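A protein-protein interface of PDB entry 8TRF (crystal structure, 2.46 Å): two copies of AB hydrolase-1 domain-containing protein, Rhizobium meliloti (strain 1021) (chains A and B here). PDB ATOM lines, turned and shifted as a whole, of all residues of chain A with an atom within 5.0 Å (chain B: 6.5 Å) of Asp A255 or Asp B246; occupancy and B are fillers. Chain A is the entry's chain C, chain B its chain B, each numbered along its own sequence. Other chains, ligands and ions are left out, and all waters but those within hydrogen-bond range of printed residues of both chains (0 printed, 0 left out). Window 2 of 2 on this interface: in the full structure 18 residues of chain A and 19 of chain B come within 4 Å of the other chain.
No position is printed for both chains. Of the 8 pairs that touch across the chains among the printed residues, none has its exchanged pair printed and touching as well.
Of the 9 printed residues of chain B, 6 touch a printed residue of chain A. Hydrophobic or aromatic side chains of chain B within 4 Å of the printed part of chain A: Ala B245 and Val B248.
The backbone NH (N) of Val B220 is in hydrogen-bond range of the backbone carbonyl oxygen (O) of Asp B247, 3.0 Å away. The backbone carbonyl oxygen of Gly A256 is in hydrogen-bond range of the backbone NH of Arg A227, at 3.0 Å. OD1 of Asp A255 lies within salt-bridge range of NH2 of Arg A262 (2.7 Å).
Of the printed residues of chain B, Arg A227 touches Ala B245 (3.96 Å). Printed residues of chain B within 4 Å of Ile A253: Val B248. Printed residues of chain B within 4 Å of Arg A254: Met B243, Pro B244 and Val B248. Of chain B, only Ala B245 (3.4 Å), Asp B246 (3.6 Å) and Asp B247 (3.9 Å) come within 4 Å of Asp A255. Printed residues of chain A within 4 Å of Ala B245: Arg A227 and Asp A255. Asp B246 touches just one residue of chain A: Asp A255 (3.6 Å). Printed residues of chain A within 4 Å of Asp B247: Asp A255. The nearest printed residue of chain B that does not touch Ile A253 is Asp B247 (6.5 Å).
The backbone carbonyl oxygen (O) of Met B243 sits at hydrogen-bond distance from the guanidinium group (NE) of Arg A254 (3.1 Å). O of Val B248 lies within hydrogen-bond range of N of Arg A254 (3.0 Å). O of Ala B245 sits close to OD2 of Asp A255, at 3.5 Å.
Among the printed residues, pairs that only touch across the chains: Arg A227 with Ala B245, Ile A253 with Val B248, Arg A254 with Pro B244, Asp A255 with Asp B246 and Asp A255 with Asp B247.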
ATOM      1  N   ARG A 227      -6.712 -10.815  -9.056  1.00  0.00           N
ATOM      2  CA  ARG A 227      -7.272 -10.875  -7.714  1.00  0.00           C
ATOM      3  C   ARG A 227      -6.586 -11.917  -6.843  1.00  0.00           C
ATOM      4  O   ARG A 227      -7.184 -12.392  -5.870  1.00  0.00           O
ATOM      5  CB  ARG A 227      -8.775 -11.147  -7.782  1.00  0.00           C
ATOM      6  CG  ARG A 227      -9.573 -10.005  -8.378  1.00  0.00           C
ATOM      7  CD  ARG A 227     -11.045 -10.363  -8.473  1.00  0.00           C
ATOM      8  NE  ARG A 227     -11.488 -11.154  -7.331  1.00  0.00           N
ATOM      9  CZ  ARG A 227     -12.421 -10.766  -6.473  1.00  0.00           C
ATOM     10  NH1 ARG A 227     -13.037  -9.603  -6.601  1.00  0.00           N
ATOM     11  NH2 ARG A 227     -12.745 -11.566  -5.460  1.00  0.00           N
ATOM     12  N   ILE A 253      -5.463 -12.783 -15.906  1.00  0.00           N
ATOM     13  CA  ILE A 253      -6.900 -12.945 -15.690  1.00  0.00           C
ATOM     14  C   ILE A 253      -7.356 -11.928 -14.654  1.00  0.00           C
ATOM     15  O   ILE A 253      -6.839 -11.899 -13.529  1.00  0.00           O
ATOM     16  CB  ILE A 253      -7.243 -14.377 -15.240  1.00  0.00           C
ATOM     17  CG1 ILE A 253      -6.483 -15.395 -16.098  1.00  0.00           C
ATOM     18  CG2 ILE A 253      -8.760 -14.606 -15.301  1.00  0.00           C
ATOM     19  CD1 ILE A 253      -6.704 -16.854 -15.723  1.00  0.00           C
ATOM     20  N   ARG A 254      -8.340 -11.106 -15.025  1.00  0.00           N
ATOM     21  CA  ARG A 254      -8.754  -9.992 -14.176  1.00  0.00           C
ATOM     22  C   ARG A 254      -9.401 -10.467 -12.878  1.00  0.00           C
ATOM     23  O   ARG A 254      -9.143  -9.896 -11.810  1.00  0.00           O
ATOM     24  CB  ARG A 254      -9.716  -9.091 -14.947  1.00  0.00           C
ATOM     25  CG  ARG A 254     -10.401  -8.039 -14.108  1.00  0.00           C
ATOM     26  CD  ARG A 254      -9.415  -7.014 -13.605  1.00  0.00           C
ATOM     27  NE  ARG A 254     -10.058  -6.039 -12.735  1.00  0.00           N
ATOM     28  CZ  ARG A 254     -10.401  -6.275 -11.477  1.00  0.00           C
ATOM     29  NH1 ARG A 254     -10.173  -7.448 -10.908  1.00  0.00           N
ATOM     30  NH2 ARG A 254     -10.981  -5.309 -10.771  1.00  0.00           N
ATOM     31  N   ASP A 255     -10.255 -11.492 -12.949  1.00  0.00           N
ATOM     32  CA  ASP A 255     -11.021 -11.955 -11.799  1.00  0.00           C
ATOM     33  C   ASP A 255     -10.468 -13.242 -11.199  1.00  0.00           C
ATOM     34  O   ASP A 255     -11.133 -13.853 -10.356  1.00  0.00           O
ATOM     35  CB  ASP A 255     -12.498 -12.144 -12.177  1.00  0.00           C
ATOM     36  CG  ASP A 255     -12.733 -13.290 -13.168  1.00  0.00           C
ATOM     37  OD1 ASP A 255     -11.761 -13.903 -13.665  1.00  0.00           O
ATOM     38  OD2 ASP A 255     -13.918 -13.572 -13.460  1.00  0.00           O
ATOM     39  N   GLY A 256      -9.275 -13.667 -11.611  1.00  0.00           N
ATOM     40  CA  GLY A 256      -8.728 -14.914 -11.118  1.00  0.00           C
ATOM     41  C   GLY A 256      -8.043 -14.752  -9.774  1.00  0.00           C
ATOM     42  O   GLY A 256      -7.459 -13.714  -9.464  1.00  0.00           O
ATOM     43  N   ASP A 257      -8.124 -15.807  -8.959  1.00  0.00           N
ATOM     44  CA  ASP A 257      -7.461 -15.795  -7.661  1.00  0.00           C
ATOM     45  C   ASP A 257      -6.163 -16.594  -7.731  1.00  0.00           C
ATOM     46  O   ASP A 257      -5.589 -16.759  -8.812  1.00  0.00           O
ATOM     47  CB  ASP A 257      -8.381 -16.337  -6.559  1.00  0.00           C
ATOM     48  CG  ASP A 257      -8.925 -17.724  -6.866  1.00  0.00           C
ATOM     49  OD1 ASP A 257      -8.455 -18.363  -7.831  1.00  0.00           O
ATOM     50  OD2 ASP A 257      -9.831 -18.179  -6.134  1.00  0.00           O
ATOM     51  N   ARG A 262     -10.983 -22.610 -11.532  1.00  0.00           N
ATOM     52  CA  ARG A 262     -12.301 -22.589 -12.146  1.00  0.00           C
ATOM     53  C   ARG A 262     -12.225 -23.193 -13.543  1.00  0.00           C
ATOM     54  O   ARG A 262     -11.150 -23.307 -14.141  1.00  0.00           O
ATOM     55  CB  ARG A 262     -12.846 -21.164 -12.219  1.00  0.00           C
ATOM     56  CG  ARG A 262     -12.983 -20.480 -10.876  1.00  0.00           C
ATOM     57  CD  ARG A 262     -13.301 -19.009 -11.055  1.00  0.00           C
ATOM     58  NE  ARG A 262     -12.288 -18.319 -11.846  1.00  0.00           N
ATOM     59  CZ  ARG A 262     -12.440 -17.105 -12.358  1.00  0.00           C
ATOM     60  NH1 ARG A 262     -13.571 -16.430 -12.209  1.00  0.00           N
ATOM     61  NH2 ARG A 262     -11.432 -16.551 -13.032  1.00  0.00           N
ATOM     62  N   GLU A 264     -13.146 -21.990 -16.376  1.00  0.00           N
ATOM     63  CA  GLU A 264     -12.585 -21.050 -17.341  1.00  0.00           C
ATOM     64  C   GLU A 264     -11.085 -20.874 -17.139  1.00  0.00           C
ATOM     65  O   GLU A 264     -10.352 -20.662 -18.111  1.00  0.00           O
ATOM     66  CB  GLU A 264     -13.303 -19.700 -17.251  1.00  0.00           C
ATOM     67  CG  GLU A 264     -13.297 -19.080 -15.864  1.00  0.00           C
ATOM     68  CD  GLU A 264     -14.628 -19.231 -15.155  1.00  0.00           C
ATOM     69  OE1 GLU A 264     -15.127 -20.374 -15.075  1.00  0.00           O
ATOM     70  OE2 GLU A 264     -15.174 -18.213 -14.675  1.00  0.00           O
ATOM     71  N   CYS B 218     -19.437  -6.759 -22.121  1.00  0.00           N
ATOM     72  CA  CYS B 218     -18.995  -7.796 -23.044  1.00  0.00           C
ATOM     73  C   CYS B 218     -17.608  -8.247 -22.620  1.00  0.00           C
ATOM     74  O   CYS B 218     -16.853  -7.451 -22.049  1.00  0.00           O
ATOM     75  CB  CYS B 218     -18.952  -7.285 -24.492  1.00  0.00           C
ATOM     76  SG  CYS B 218     -17.721  -5.977 -24.752  1.00  0.00           S
ATOM     77  N   PRO B 219     -17.235  -9.499 -22.891  1.00  0.00           N
ATOM     78  CA  PRO B 219     -15.869  -9.937 -22.576  1.00  0.00           C
ATOM     79  C   PRO B 219     -14.842  -9.088 -23.310  1.00  0.00           C
ATOM     80  O   PRO B 219     -15.092  -8.575 -24.404  1.00  0.00           O
ATOM     81  CB  PRO B 219     -15.839 -11.396 -23.048  1.00  0.00           C
ATOM     82  CG  PRO B 219     -16.999 -11.532 -23.987  1.00  0.00           C
ATOM     83  CD  PRO B 219     -18.040 -10.572 -23.499  1.00  0.00           C
ATOM     84  N   VAL B 220     -13.678  -8.923 -22.685  1.00  0.00           N
ATOM     85  CA  VAL B 220     -12.627  -8.057 -23.203  1.00  0.00           C
ATOM     86  C   VAL B 220     -11.315  -8.829 -23.206  1.00  0.00           C
ATOM     87  O   VAL B 220     -10.940  -9.427 -22.191  1.00  0.00           O
ATOM     88  CB  VAL B 220     -12.493  -6.769 -22.366  1.00  0.00           C
ATOM     89  CG1 VAL B 220     -11.253  -5.977 -22.791  1.00  0.00           C
ATOM     90  CG2 VAL B 220     -13.756  -5.924 -22.482  1.00  0.00           C
ATOM     91  N   MET B 243     -11.851  -2.177 -14.536  1.00  0.00           N
ATOM     92  CA  MET B 243     -12.899  -2.990 -15.134  1.00  0.00           C
ATOM     93  C   MET B 243     -13.387  -4.062 -14.162  1.00  0.00           C
ATOM     94  O   MET B 243     -12.659  -4.458 -13.245  1.00  0.00           O
ATOM     95  CB  MET B 243     -12.385  -3.632 -16.432  1.00  0.00           C
ATOM     96  CG  MET B 243     -11.949  -2.596 -17.469  1.00  0.00           C
ATOM     97  SD  MET B 243     -11.430  -3.264 -19.068  1.00  0.00           S
ATOM     98  CE  MET B 243     -12.998  -3.833 -19.706  1.00  0.00           C
ATOM     99  N   PRO B 244     -14.636  -4.560 -14.326  1.00  0.00           N
ATOM    100  CA  PRO B 244     -15.204  -5.461 -13.314  1.00  0.00           C
ATOM    101  C   PRO B 244     -14.471  -6.785 -13.206  1.00  0.00           C
ATOM    102  O   PRO B 244     -13.551  -7.070 -13.979  1.00  0.00           O
ATOM    103  CB  PRO B 244     -16.643  -5.673 -13.809  1.00  0.00           C
ATOM    104  CG  PRO B 244     -16.910  -4.501 -14.698  1.00  0.00           C
ATOM    105  CD  PRO B 244     -15.604  -4.332 -15.410  1.00  0.00           C
ATOM    106  N   ALA B 245     -14.889  -7.610 -12.248  1.00  0.00           N
ATOM    107  CA  ALA B 245     -14.279  -8.920 -12.038  1.00  0.00           C
ATOM    108  C   ALA B 245     -15.052  -9.972 -12.835  1.00  0.00           C
ATOM    109  O   ALA B 245     -15.720 -10.856 -12.290  1.00  0.00           O
ATOM    110  CB  ALA B 245     -14.229  -9.252 -10.552  1.00  0.00           C
ATOM    111  N   ASP B 246     -14.949  -9.857 -14.161  1.00  0.00           N
ATOM    112  CA  ASP B 246     -15.570 -10.828 -15.060  1.00  0.00           C
ATOM    113  C   ASP B 246     -14.992 -10.675 -16.459  1.00  0.00           C
ATOM    114  O   ASP B 246     -15.165  -9.626 -17.091  1.00  0.00           O
ATOM    115  CB  ASP B 246     -17.091 -10.660 -15.089  1.00  0.00           C
ATOM    116  CG  ASP B 246     -17.801 -11.890 -15.627  1.00  0.00           C
ATOM    117  OD1 ASP B 246     -17.271 -13.009 -15.458  1.00  0.00           O
ATOM    118  OD2 ASP B 246     -18.893 -11.738 -16.214  1.00  0.00           O
ATOM    119  N   ASP B 247     -14.310 -11.721 -16.927  1.00  0.00           N
ATOM    120  CA  ASP B 247     -13.885 -11.902 -18.317  1.00  0.00           C
ATOM    121  C   ASP B 247     -13.224 -10.654 -18.900  1.00  0.00           C
ATOM    122  O   ASP B 247     -13.675 -10.065 -19.886  1.00  0.00           O
ATOM    123  CB  ASP B 247     -15.050 -12.353 -19.196  1.00  0.00           C
ATOM    124  CG  ASP B 247     -14.605 -13.316 -20.279  1.00  0.00           C
ATOM    125  OD1 ASP B 247     -13.376 -13.446 -20.478  1.00  0.00           O
ATOM    126  OD2 ASP B 247     -15.469 -13.946 -20.925  1.00  0.00           O
ATOM    127  N   VAL B 248     -12.126 -10.264 -18.270  1.00  0.00           N
ATOM    128  CA  VAL B 248     -11.180  -9.327 -18.848  1.00  0.00           C
ATOM    129  C   VAL B 248      -9.833 -10.036 -18.809  1.00  0.00           C
ATOM    130  O   VAL B 248      -9.329 -10.360 -17.727  1.00  0.00           O
ATOM    131  CB  VAL B 248     -11.137  -7.991 -18.096  1.00  0.00           C
ATOM    132  CG1 VAL B 248     -10.182  -7.034 -18.784  1.00  0.00           C
ATOM    133  CG2 VAL B 248     -12.531  -7.388 -18.012  1.00  0.00           C
